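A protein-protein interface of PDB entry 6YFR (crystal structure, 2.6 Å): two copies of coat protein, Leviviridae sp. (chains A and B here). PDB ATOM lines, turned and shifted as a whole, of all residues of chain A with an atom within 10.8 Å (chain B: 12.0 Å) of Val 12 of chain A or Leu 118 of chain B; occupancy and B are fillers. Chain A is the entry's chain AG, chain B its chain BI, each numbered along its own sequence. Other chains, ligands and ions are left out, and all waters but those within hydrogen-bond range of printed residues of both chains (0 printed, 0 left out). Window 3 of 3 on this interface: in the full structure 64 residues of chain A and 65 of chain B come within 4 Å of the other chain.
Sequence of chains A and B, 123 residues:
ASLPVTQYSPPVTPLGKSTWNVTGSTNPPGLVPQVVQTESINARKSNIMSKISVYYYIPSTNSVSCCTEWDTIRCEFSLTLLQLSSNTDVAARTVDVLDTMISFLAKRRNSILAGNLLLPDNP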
ATOM      1  N   GLN A   7      38.815 -16.978 -22.813  1.00  0.00           N
ATOM      2  CA  GLN A   7      38.354 -17.850 -21.744  1.00  0.00           C
ATOM      3  C   GLN A   7      39.540 -18.543 -21.085  1.00  0.00           C
ATOM      4  O   GLN A   7      40.254 -19.315 -21.732  1.00  0.00           O
ATOM      5  CB  GLN A   7      37.366 -18.875 -22.285  1.00  0.00           C
ATOM      6  CG  GLN A   7      36.628 -19.620 -21.195  1.00  0.00           C
ATOM      7  CD  GLN A   7      35.225 -19.995 -21.609  1.00  0.00           C
ATOM      8  OE1 GLN A   7      34.258 -19.668 -20.921  1.00  0.00           O
ATOM      9  NE2 GLN A   7      35.102 -20.687 -22.739  1.00  0.00           N
ATOM     10  N   TYR A   8      39.739 -18.267 -19.795  1.00  0.00           N
ATOM     11  CA  TYR A   8      40.816 -18.845 -18.998  1.00  0.00           C
ATOM     12  C   TYR A   8      40.398 -20.162 -18.348  1.00  0.00           C
ATOM     13  O   TYR A   8      41.019 -21.201 -18.595  1.00  0.00           O
ATOM     14  CB  TYR A   8      41.275 -17.823 -17.949  1.00  0.00           C
ATOM     15  CG  TYR A   8      42.198 -18.340 -16.864  1.00  0.00           C
ATOM     16  CD1 TYR A   8      43.473 -18.813 -17.163  1.00  0.00           C
ATOM     17  CD2 TYR A   8      41.802 -18.317 -15.530  1.00  0.00           C
ATOM     18  CE1 TYR A   8      44.318 -19.273 -16.159  1.00  0.00           C
ATOM     19  CE2 TYR A   8      42.634 -18.770 -14.524  1.00  0.00           C
ATOM     20  CZ  TYR A   8      43.890 -19.246 -14.840  1.00  0.00           C
ATOM     21  OH  TYR A   8      44.712 -19.696 -13.832  1.00  0.00           O
ATOM     22  N   SER A   9      39.345 -20.146 -17.532  1.00  0.00           N
ATOM     23  CA  SER A   9      38.797 -21.381 -16.977  1.00  0.00           C
ATOM     24  C   SER A   9      37.451 -21.678 -17.620  1.00  0.00           C
ATOM     25  O   SER A   9      36.474 -20.960 -17.358  1.00  0.00           O
ATOM     26  CB  SER A   9      38.647 -21.285 -15.459  1.00  0.00           C
ATOM     27  OG  SER A   9      38.024 -22.454 -14.944  1.00  0.00           O
ATOM     28  N   PRO A  10      37.343 -22.716 -18.440  1.00  0.00           N
ATOM     29  CA  PRO A  10      36.124 -22.930 -19.220  1.00  0.00           C
ATOM     30  C   PRO A  10      35.032 -23.544 -18.366  1.00  0.00           C
ATOM     31  O   PRO A  10      35.303 -24.053 -17.265  1.00  0.00           O
ATOM     32  CB  PRO A  10      36.586 -23.898 -20.317  1.00  0.00           C
ATOM     33  CG  PRO A  10      37.635 -24.713 -19.632  1.00  0.00           C
ATOM     34  CD  PRO A  10      38.331 -23.784 -18.662  1.00  0.00           C
ATOM     35  N   PRO A  11      33.779 -23.500 -18.821  1.00  0.00           N
ATOM     36  CA  PRO A  11      32.698 -24.110 -18.042  1.00  0.00           C
ATOM     37  C   PRO A  11      32.833 -25.621 -18.005  1.00  0.00           C
ATOM     38  O   PRO A  11      33.171 -26.268 -19.001  1.00  0.00           O
ATOM     39  CB  PRO A  11      31.429 -23.669 -18.780  1.00  0.00           C
ATOM     40  CG  PRO A  11      31.880 -23.411 -20.170  1.00  0.00           C
ATOM     41  CD  PRO A  11      33.267 -22.843 -20.037  1.00  0.00           C
ATOM     42  N   VAL A  12      32.559 -26.173 -16.835  1.00  0.00           N
ATOM     43  CA  VAL A  12      32.738 -27.585 -16.559  1.00  0.00           C
ATOM     44  C   VAL A  12      31.395 -28.290 -16.421  1.00  0.00           C
ATOM     45  O   VAL A  12      31.129 -29.293 -17.086  1.00  0.00           O
ATOM     46  CB  VAL A  12      33.598 -27.767 -15.290  1.00  0.00           C
ATOM     47  CG1 VAL A  12      33.776 -29.222 -14.962  1.00  0.00           C
ATOM     48  CG2 VAL A  12      34.938 -27.044 -15.451  1.00  0.00           C
ATOM     49  N   THR A  13      30.528 -27.758 -15.572  1.00  0.00           N
ATOM     50  CA  THR A  13      29.194 -28.255 -15.311  1.00  0.00           C
ATOM     51  C   THR A  13      28.217 -27.096 -15.421  1.00  0.00           C
ATOM     52  O   THR A  13      28.627 -25.930 -15.387  1.00  0.00           O
ATOM     53  CB  THR A  13      29.117 -28.891 -13.915  1.00  0.00           C
ATOM     54  OG1 THR A  13      29.553 -27.941 -12.937  1.00  0.00           O
ATOM     55  CG2 THR A  13      30.001 -30.130 -13.849  1.00  0.00           C
ATOM     56  N   PRO A  14      26.919 -27.375 -15.575  1.00  0.00           N
ATOM     57  CA  PRO A  14      25.936 -26.279 -15.640  1.00  0.00           C
ATOM     58  C   PRO A  14      26.012 -25.312 -14.468  1.00  0.00           C
ATOM     59  O   PRO A  14      25.821 -24.103 -14.655  1.00  0.00           O
ATOM     60  CB  PRO A  14      24.589 -27.024 -15.682  1.00  0.00           C
ATOM     61  CG  PRO A  14      24.903 -28.427 -15.241  1.00  0.00           C
ATOM     62  CD  PRO A  14      26.272 -28.682 -15.751  1.00  0.00           C
ATOM     63  N   LEU A  15      26.297 -25.807 -13.271  1.00  0.00           N
ATOM     64  CA  LEU A  15      26.514 -24.952 -12.114  1.00  0.00           C
ATOM     65  C   LEU A  15      28.006 -24.805 -11.848  1.00  0.00           C
ATOM     66  O   LEU A  15      28.810 -25.667 -12.213  1.00  0.00           O
ATOM     67  CB  LEU A  15      25.815 -25.519 -10.882  1.00  0.00           C
ATOM     68  CG  LEU A  15      24.326 -25.799 -11.082  1.00  0.00           C
ATOM     69  CD1 LEU A  15      23.781 -26.548  -9.884  1.00  0.00           C
ATOM     70  CD2 LEU A  15      23.571 -24.500 -11.304  1.00  0.00           C
ATOM     71  N   GLY A  16      28.370 -23.694 -11.213  1.00  0.00           N
ATOM     72  CA  GLY A  16      29.761 -23.429 -10.910  1.00  0.00           C
ATOM     73  C   GLY A  16      30.222 -22.072 -11.396  1.00  0.00           C
ATOM     74  O   GLY A  16      29.442 -21.111 -11.410  1.00  0.00           O
ATOM     75  N   LYS A  17      31.485 -21.992 -11.823  1.00  0.00           N
ATOM     76  CA  LYS A  17      32.105 -20.745 -12.251  1.00  0.00           C
ATOM     77  C   LYS A  17      32.825 -20.940 -13.575  1.00  0.00           C
ATOM     78  O   LYS A  17      33.394 -22.003 -13.836  1.00  0.00           O
ATOM     79  CB  LYS A  17      33.111 -20.219 -11.211  1.00  0.00           C
ATOM     80  CG  LYS A  17      32.493 -19.660  -9.940  1.00  0.00           C
ATOM     81  CD  LYS A  17      33.522 -18.881  -9.123  1.00  0.00           C
ATOM     82  CE  LYS A  17      34.717 -19.748  -8.740  1.00  0.00           C
ATOM     83  NZ  LYS A  17      35.682 -19.029  -7.859  1.00  0.00           N
ATOM     84  N   SER A  18      32.799 -19.898 -14.401  1.00  0.00           N
ATOM     85  CA  SER A  18      33.596 -19.810 -15.613  1.00  0.00           C
ATOM     86  C   SER A  18      34.275 -18.448 -15.618  1.00  0.00           C
ATOM     87  O   SER A  18      33.670 -17.455 -15.206  1.00  0.00           O
ATOM     88  CB  SER A  18      32.731 -19.993 -16.865  1.00  0.00           C
ATOM     89  OG  SER A  18      33.429 -19.608 -18.035  1.00  0.00           O
ATOM     90  N   THR A  19      35.535 -18.394 -16.057  1.00  0.00           N
ATOM     91  CA  THR A  19      36.290 -17.146 -16.003  1.00  0.00           C
ATOM     92  C   THR A  19      36.956 -16.844 -17.337  1.00  0.00           C
ATOM     93  O   THR A  19      37.507 -17.734 -17.993  1.00  0.00           O
ATOM     94  CB  THR A  19      37.362 -17.169 -14.898  1.00  0.00           C
ATOM     95  OG1 THR A  19      38.343 -18.167 -15.196  1.00  0.00           O
ATOM     96  CG2 THR A  19      36.739 -17.461 -13.539  1.00  0.00           C
ATOM     97  N   TRP A  20      36.894 -15.572 -17.721  1.00  0.00           N
ATOM     98  CA  TRP A  20      37.625 -15.010 -18.846  1.00  0.00           C
ATOM     99  C   TRP A  20      38.659 -14.023 -18.321  1.00  0.00           C
ATOM    100  O   TRP A  20      38.397 -13.291 -17.357  1.00  0.00           O
ATOM    101  CB  TRP A  20      36.694 -14.274 -19.811  1.00  0.00           C
ATOM    102  CG  TRP A  20      35.641 -15.115 -20.445  1.00  0.00           C
ATOM    103  CD1 TRP A  20      35.635 -15.588 -21.724  1.00  0.00           C
ATOM    104  CD2 TRP A  20      34.425 -15.572 -19.841  1.00  0.00           C
ATOM    105  NE1 TRP A  20      34.494 -16.317 -21.955  1.00  0.00           N
ATOM    106  CE2 TRP A  20      33.734 -16.322 -20.816  1.00  0.00           C
ATOM    107  CE3 TRP A  20      33.855 -15.426 -18.574  1.00  0.00           C
ATOM    108  CZ2 TRP A  20      32.505 -16.922 -20.560  1.00  0.00           C
ATOM    109  CZ3 TRP A  20      32.631 -16.024 -18.325  1.00  0.00           C
ATOM    110  CH2 TRP A  20      31.971 -16.760 -19.312  1.00  0.00           C
ATOM    111  N   GLN A  37      31.517 -15.646 -14.641  1.00  0.00           N
ATOM    112  CA  GLN A  37      30.108 -16.017 -14.653  1.00  0.00           C
ATOM    113  C   GLN A  37      29.882 -17.152 -13.665  1.00  0.00           C
ATOM    114  O   GLN A  37      30.617 -18.144 -13.669  1.00  0.00           O
ATOM    115  CB  GLN A  37      29.638 -16.441 -16.046  1.00  0.00           C
ATOM    116  CG  GLN A  37      28.176 -16.863 -16.062  1.00  0.00           C
ATOM    117  CD  GLN A  37      27.730 -17.447 -17.390  1.00  0.00           C
ATOM    118  OE1 GLN A  37      28.486 -17.475 -18.363  1.00  0.00           O
ATOM    119  NE2 GLN A  37      26.487 -17.921 -17.434  1.00  0.00           N
ATOM    120  N   THR A  38      28.862 -17.004 -12.829  1.00  0.00           N
ATOM    121  CA  THR A  38      28.544 -17.955 -11.773  1.00  0.00           C
ATOM    122  C   THR A  38      27.105 -18.420 -11.937  1.00  0.00           C
ATOM    123  O   THR A  38      26.216 -17.607 -12.201  1.00  0.00           O
ATOM    124  CB  THR A  38      28.740 -17.322 -10.391  1.00  0.00           C
ATOM    125  OG1 THR A  38      30.135 -17.095 -10.165  1.00  0.00           O
ATOM    126  CG2 THR A  38      28.185 -18.214  -9.293  1.00  0.00           C
ATOM    127  N   GLU A  39      26.879 -19.724 -11.803  1.00  0.00           N
ATOM    128  CA  GLU A  39      25.529 -20.284 -11.779  1.00  0.00           C
ATOM    129  C   GLU A  39      25.414 -21.156 -10.537  1.00  0.00           C
ATOM    130  O   GLU A  39      25.978 -22.253 -10.490  1.00  0.00           O
ATOM    131  CB  GLU A  39      25.232 -21.082 -13.049  1.00  0.00           C
ATOM    132  CG  GLU A  39      25.309 -20.264 -14.328  1.00  0.00           C
ATOM    133  CD  GLU A  39      24.263 -19.164 -14.396  1.00  0.00           C
ATOM    134  OE1 GLU A  39      23.240 -19.258 -13.685  1.00  0.00           O
ATOM    135  OE2 GLU A  39      24.464 -18.204 -15.168  1.00  0.00           O
ATOM    136  N   SER A  50      22.119 -16.490 -11.405  1.00  0.00           N
ATOM    137  CA  SER A  50      23.022 -16.255 -12.524  1.00  0.00           C
ATOM    138  C   SER A  50      23.740 -14.936 -12.275  1.00  0.00           C
ATOM    139  O   SER A  50      23.091 -13.891 -12.165  1.00  0.00           O
ATOM    140  CB  SER A  50      22.265 -16.205 -13.851  1.00  0.00           C
ATOM    141  OG  SER A  50      21.617 -17.431 -14.134  1.00  0.00           O
ATOM    142  N   LYS B 107      26.495 -11.851 -24.620  1.00  0.00           N
ATOM    143  CA  LYS B 107      27.226 -13.052 -25.006  1.00  0.00           C
ATOM    144  C   LYS B 107      26.676 -14.297 -24.322  1.00  0.00           C
ATOM    145  O   LYS B 107      26.602 -15.368 -24.936  1.00  0.00           O
ATOM    146  CB  LYS B 107      28.701 -12.854 -24.663  1.00  0.00           C
ATOM    147  CG  LYS B 107      29.591 -14.067 -24.808  1.00  0.00           C
ATOM    148  CD  LYS B 107      30.978 -13.759 -24.248  1.00  0.00           C
ATOM    149  CE  LYS B 107      31.986 -14.833 -24.616  1.00  0.00           C
ATOM    150  NZ  LYS B 107      33.334 -14.576 -24.050  1.00  0.00           N
ATOM    151  N   ARG B 108      26.278 -14.178 -23.057  1.00  0.00           N
ATOM    152  CA  ARG B 108      25.869 -15.318 -22.248  1.00  0.00           C
ATOM    153  C   ARG B 108      24.385 -15.281 -21.897  1.00  0.00           C
ATOM    154  O   ARG B 108      23.988 -15.763 -20.836  1.00  0.00           O
ATOM    155  CB  ARG B 108      26.704 -15.377 -20.971  1.00  0.00           C
ATOM    156  CG  ARG B 108      28.204 -15.295 -21.196  1.00  0.00           C
ATOM    157  CD  ARG B 108      28.704 -16.543 -21.898  1.00  0.00           C
ATOM    158  NE  ARG B 108      28.332 -17.749 -21.166  1.00  0.00           N
ATOM    159  CZ  ARG B 108      28.250 -18.955 -21.716  1.00  0.00           C
ATOM    160  NH1 ARG B 108      28.510 -19.115 -23.008  1.00  0.00           N
ATOM    161  NH2 ARG B 108      27.902 -20.002 -20.976  1.00  0.00           N
ATOM    162  N   ARG B 109      23.554 -14.707 -22.771  1.00  0.00           N
ATOM    163  CA  ARG B 109      22.140 -14.534 -22.443  1.00  0.00           C
ATOM    164  C   ARG B 109      21.453 -15.872 -22.187  1.00  0.00           C
ATOM    165  O   ARG B 109      20.729 -16.032 -21.196  1.00  0.00           O
ATOM    166  CB  ARG B 109      21.435 -13.771 -23.565  1.00  0.00           C
ATOM    167  CG  ARG B 109      19.928 -13.819 -23.470  1.00  0.00           C
ATOM    168  CD  ARG B 109      19.294 -12.688 -24.252  1.00  0.00           C
ATOM    169  NE  ARG B 109      17.983 -12.349 -23.709  1.00  0.00           N
ATOM    170  CZ  ARG B 109      17.322 -11.234 -23.993  1.00  0.00           C
ATOM    171  NH1 ARG B 109      17.845 -10.345 -24.824  1.00  0.00           N
ATOM    172  NH2 ARG B 109      16.132 -11.016 -23.450  1.00  0.00           N
ATOM    173  N   ASN B 110      21.660 -16.847 -23.075  1.00  0.00           N
ATOM    174  CA  ASN B 110      21.008 -18.140 -22.896  1.00  0.00           C
ATOM    175  C   ASN B 110      21.491 -18.827 -21.626  1.00  0.00           C
ATOM    176  O   ASN B 110      20.685 -19.384 -20.871  1.00  0.00           O
ATOM    177  CB  ASN B 110      21.261 -19.034 -24.108  1.00  0.00           C
ATOM    178  CG  ASN B 110      20.773 -18.416 -25.400  1.00  0.00           C
ATOM    179  OD1 ASN B 110      19.851 -17.600 -25.400  1.00  0.00           O
ATOM    180  ND2 ASN B 110      21.398 -18.793 -26.510  1.00  0.00           N
ATOM    181  N   SER B 111      22.802 -18.798 -21.376  1.00  0.00           N
ATOM    182  CA  SER B 111      23.339 -19.415 -20.169  1.00  0.00           C
ATOM    183  C   SER B 111      22.764 -18.762 -18.917  1.00  0.00           C
ATOM    184  O   SER B 111      22.385 -19.451 -17.961  1.00  0.00           O
ATOM    185  CB  SER B 111      24.864 -19.322 -20.172  1.00  0.00           C
ATOM    186  OG  SER B 111      25.414 -19.983 -19.050  1.00  0.00           O
ATOM    187  N   ILE B 112      22.687 -17.428 -18.912  1.00  0.00           N
ATOM    188  CA  ILE B 112      22.156 -16.700 -17.764  1.00  0.00           C
ATOM    189  C   ILE B 112      20.691 -17.051 -17.540  1.00  0.00           C
ATOM    190  O   ILE B 112      20.249 -17.254 -16.400  1.00  0.00           O
ATOM    191  CB  ILE B 112      22.352 -15.184 -17.958  1.00  0.00           C
ATOM    192  CG1 ILE B 112      23.834 -14.827 -17.855  1.00  0.00           C
ATOM    193  CG2 ILE B 112      21.539 -14.398 -16.949  1.00  0.00           C
ATOM    194  CD1 ILE B 112      24.127 -13.387 -18.182  1.00  0.00           C
ATOM    195  N   LEU B 113      19.913 -17.129 -18.622  1.00  0.00           N
ATOM    196  CA  LEU B 113      18.482 -17.374 -18.489  1.00  0.00           C
ATOM    197  C   LEU B 113      18.170 -18.825 -18.162  1.00  0.00           C
ATOM    198  O   LEU B 113      17.109 -19.108 -17.594  1.00  0.00           O
ATOM    199  CB  LEU B 113      17.749 -16.967 -19.771  1.00  0.00           C
ATOM    200  CG  LEU B 113      17.682 -15.467 -20.066  1.00  0.00           C
ATOM    201  CD1 LEU B 113      16.989 -15.235 -21.391  1.00  0.00           C
ATOM    202  CD2 LEU B 113      16.960 -14.738 -18.952  1.00  0.00           C
ATOM    203  N   ALA B 114      19.064 -19.753 -18.500  1.00  0.00           N
ATOM    204  CA  ALA B 114      18.816 -21.168 -18.257  1.00  0.00           C
ATOM    205  C   ALA B 114      19.501 -21.702 -17.003  1.00  0.00           C
ATOM    206  O   ALA B 114      19.159 -22.802 -16.558  1.00  0.00           O
ATOM    207  CB  ALA B 114      19.257 -21.992 -19.475  1.00  0.00           C
ATOM    208  N   GLY B 115      20.443 -20.962 -16.426  1.00  0.00           N
ATOM    209  CA  GLY B 115      21.167 -21.476 -15.275  1.00  0.00           C
ATOM    210  C   GLY B 115      22.075 -22.632 -15.628  1.00  0.00           C
ATOM    211  O   GLY B 115      22.158 -23.607 -14.868  1.00  0.00           O
ATOM    212  N   ASN B 116      22.755 -22.551 -16.771  1.00  0.00           N
ATOM    213  CA  ASN B 116      23.613 -23.626 -17.262  1.00  0.00           C
ATOM    214  C   ASN B 116      24.855 -22.996 -17.879  1.00  0.00           C
ATOM    215  O   ASN B 116      24.766 -22.344 -18.925  1.00  0.00           O
ATOM    216  CB  ASN B 116      22.870 -24.490 -18.282  1.00  0.00           C
ATOM    217  CG  ASN B 116      23.585 -25.792 -18.579  1.00  0.00           C
ATOM    218  OD1 ASN B 116      24.814 -25.843 -18.647  1.00  0.00           O
ATOM    219  ND2 ASN B 116      22.813 -26.860 -18.757  1.00  0.00           N
ATOM    220  N   LEU B 117      26.010 -23.197 -17.238  1.00  0.00           N
ATOM    221  CA  LEU B 117      27.259 -22.625 -17.731  1.00  0.00           C
ATOM    222  C   LEU B 117      27.699 -23.224 -19.056  1.00  0.00           C
ATOM    223  O   LEU B 117      28.491 -22.599 -19.769  1.00  0.00           O
ATOM    224  CB  LEU B 117      28.378 -22.827 -16.712  1.00  0.00           C
ATOM    225  CG  LEU B 117      28.336 -22.001 -15.434  1.00  0.00           C
ATOM    226  CD1 LEU B 117      29.317 -22.577 -14.446  1.00  0.00           C
ATOM    227  CD2 LEU B 117      28.683 -20.565 -15.749  1.00  0.00           C
ATOM    228  N   LEU B 118      27.219 -24.419 -19.397  1.00  0.00           N
ATOM    229  CA  LEU B 118      27.736 -25.137 -20.553  1.00  0.00           C
ATOM    230  C   LEU B 118      27.147 -24.670 -21.874  1.00  0.00           C
ATOM    231  O   LEU B 118      27.664 -25.057 -22.927  1.00  0.00           O
ATOM    232  CB  LEU B 118      27.483 -26.635 -20.389  1.00  0.00           C
ATOM    233  CG  LEU B 118      28.141 -27.291 -19.177  1.00  0.00           C
ATOM    234  CD1 LEU B 118      27.665 -28.715 -19.044  1.00  0.00           C
ATOM    235  CD2 LEU B 118      29.654 -27.242 -19.308  1.00  0.00           C
ATOM    236  N   LEU B 119      26.085 -23.872 -21.855  1.00  0.00           N
ATOM    237  CA  LEU B 119      25.490 -23.421 -23.103  1.00  0.00           C
ATOM    238  C   LEU B 119      26.480 -22.537 -23.859  1.00  0.00           C
ATOM    239  O   LEU B 119      27.170 -21.713 -23.247  1.00  0.00           O
ATOM    240  CB  LEU B 119      24.194 -22.649 -22.850  1.00  0.00           C
ATOM    241  CG  LEU B 119      23.079 -23.402 -22.127  1.00  0.00           C
ATOM    242  CD1 LEU B 119      21.811 -22.567 -22.101  1.00  0.00           C
ATOM    243  CD2 LEU B 119      22.833 -24.741 -22.794  1.00  0.00           C
ATOM    244  N   PRO B 120      26.581 -22.685 -25.174  1.00  0.00           N
ATOM    245  CA  PRO B 120      27.495 -21.837 -25.945  1.00  0.00           C
ATOM    246  C   PRO B 120      27.045 -20.385 -25.922  1.00  0.00           C
ATOM    247  O   PRO B 120      25.917 -20.057 -25.548  1.00  0.00           O
ATOM    248  CB  PRO B 120      27.419 -22.426 -27.356  1.00  0.00           C
ATOM    249  CG  PRO B 120      26.078 -23.091 -27.413  1.00  0.00           C
ATOM    250  CD  PRO B 120      25.822 -23.615 -26.028  1.00  0.00           C
ATOM    251  N   ASP B 121      27.962 -19.508 -26.325  1.00  0.00           N
ATOM    252  CA  ASP B 121      27.638 -18.094 -26.443  1.00  0.00           C
ATOM    253  C   ASP B 121      26.430 -17.902 -27.351  1.00  0.00           C
ATOM    254  O   ASP B 121      26.203 -18.669 -28.291  1.00  0.00           O
ATOM    255  CB  ASP B 121      28.823 -17.307 -27.005  1.00  0.00           C
ATOM    256  CG  ASP B 121      30.010 -17.279 -26.068  1.00  0.00           C
ATOM    257  OD1 ASP B 121      29.829 -17.508 -24.853  1.00  0.00           O
ATOM    258  OD2 ASP B 121      31.132 -17.016 -26.555  1.00  0.00           O
ATOM    259  N   ASN B 122      25.644 -16.877 -27.051  1.00  0.00           N
ATOM    260  CA  ASN B 122      24.551 -16.512 -27.935  1.00  0.00           C
ATOM    261  C   ASN B 122      25.110 -16.105 -29.297  1.00  0.00           C
ATOM    262  O   ASN B 122      26.167 -15.466 -29.367  1.00  0.00           O
ATOM    263  CB  ASN B 122      23.731 -15.368 -27.339  1.00  0.00           C
ATOM    264  CG  ASN B 122      22.715 -15.845 -26.319  1.00  0.00           C
ATOM    265  OD1 ASN B 122      23.071 -16.295 -25.228  1.00  0.00           O
ATOM    266  ND2 ASN B 122      21.439 -15.736 -26.665  1.00  0.00           N
ATOM    267  N   PRO B 123      24.438 -16.465 -30.398  1.00  0.00           N
ATOM    268  CA  PRO B 123      24.878 -16.042 -31.730  1.00  0.00           C
ATOM    269  C   PRO B 123      24.773 -14.530 -31.906  1.00  0.00           C
ATOM    270  O   PRO B 123      23.768 -13.918 -31.539  1.00  0.00           O
ATOM    271  CB  PRO B 123      23.916 -16.776 -32.666  1.00  0.00           C
ATOM    272  CG  PRO B 123      22.703 -17.037 -31.832  1.00  0.00           C
ATOM    273  CD  PRO B 123      23.221 -17.293 -30.452  1.00  0.00           C
ATOM    274  OXT PRO B 123      25.691 -13.886 -32.412  1.00  0.00           O
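N of Leu 117 of chain B sits at hydrogen-bond distance from O of Pro 14 of chain A, at 2.7 Å. NE1 of Trp 20 of chain A sits close to NZ of Lys 107 of chain B, 3.0 Å away. The backbone carbonyl oxygen (O) of Ile 112 of chain B sits at hydrogen-bond distance from the side-chain hydroxyl (OG) of Ser 50 of chain A (2.7 Å). NE of Arg 108 of chain B is in hydrogen-bond range of OE1 of Gln 37 of chain A. OG of Ser 111 of chain B is in hydrogen-bond range of NE2 of Gln 37 of chain A (2.8 Å).
OG of Ser 50 of chain A sits at hydrogen-bond distance from OE1 of Glu 39 of chain A (2.5 Å). OG of Ser 111 of chain B lies within hydrogen-bond range of O of Asn 116 of chain B, at 2.5 Å. The backbone carbonyl oxygen (O) of Leu 15 of chain A sits at hydrogen-bond distance from the side-chain hydroxyl (OG1) of Thr 13 of chain A, 2.5 Å away. The backbone carbonyl oxygen (O) of Glu 39 of chain A is in hydrogen-bond range of the backbone NH (N) of Gly 16 of chain A (2.9 Å). The backbone NH (N) of Asn 122 of chain B sits at hydrogen-bond distance from the backbone carbonyl oxygen (O) of Lys 107 of chain B, 2.8 Å away. The guanidinium group (NH2) of Arg 108 of chain B sits at hydrogen-bond distance from the side-chain hydroxyl (OG) of Ser 111 of chain B.
Among the printed residues, pairs that only touch across the chains: Pro 11 of chain A with Leu 117 of chain B, Pro 11 of chain A with Leu 118 of chain B, Val 12 of chain A with Leu 118 of chain B, Thr 13 of chain A with Leu 117 of chain B, Thr 13 of chain A with Leu 118 of chain B, Pro 14 of chain A with Gly 115 of chain B, Pro 14 of chain A with Asn 116 of chain B, Pro 14 of chain A with Leu 118 of chain B, Leu 15 of chain A with Gly 115 of chain B, Leu 15 of chain A with Leu 117 of chain B, Gly 16 of chain A with Leu 117 of chain B, Lys 17 of chain A with Leu 117 of chain B, Gln 37 of chain A with Leu 117 of chain B, Glu 39 of chain A with Ser 111 of chain B, Glu 39 of chain A with Ile 112 of chain B, Glu 39 of chain A with Gly 115 of chain B and Glu 39 of chain A with Leu 117 of chain B.
Val 12 of chain A touches just one residue of chain B: Leu 118. Leu 118 of chain B touches just these residues of chain A: Pro 11 (3.7 Å), Val 12 (3.4 Å), Thr 13 (3.8 Å) and Pro 14 (3.6 Å). Pro 14 of chain A touches four residues of chain B. Of chain A, only Pro 14 comes within 4 Å of Asn 116 of chain B. Of chain A, only Pro 11 (3.3 Å), Thr 13 (3.4 Å), Pro 14 (2.7 Å), Leu 15 (3.7 Å), Gly 16 (3.2 Å), Lys 17 (3.5 Å), Gln 37 (3.7 Å) and Glu 39 (3.7 Å) come within 4 Å of Leu 117 of chain B. No residue of chain A comes within 4 Å of Leu 119 of chain B. No residue of chain A comes within 4 Å of Pro 120 of chain B. Of the printed residues of chain B, Gln 37 of chain A touches Arg 108 (2.8 Å), Ser 111 (2.8 Å) and Leu 117 (3.7 Å). Of the printed residues of chain A, Ser 111 of chain B touches Gln 37 (2.8 Å) and Glu 39 (3.7 Å). Printed residues of chain B within 4 Å of Gly 16 of chain A: Leu 117 (3.2 Å). Of the printed residues of chain B, Ser 50 of chain A touches Ile 112 (2.7 Å). Leu 113 of chain B touches none of the printed residues of chain A. The nearest printed residue of chain B that does not touch Leu 15 of chain A is Asn 116 of chain B (5.3 Å).
Of the 17 printed residues of chain B, 8 touch a printed residue of chain A. Hydrophobic or aromatic side chains of chain A that line the printed part of chain B: Pro 11, Pro 14, Leu 15 and Trp 20. Along chain A the printed residues that touch a printed residue of chain B span positions 11 to 50. Among the printed residues, 22 pairs touch across the chains.
No position is printed for both chains. Of the 22 pairs that touch across the chains among the printed residues, none has its exchanged pair printed and touching as well.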
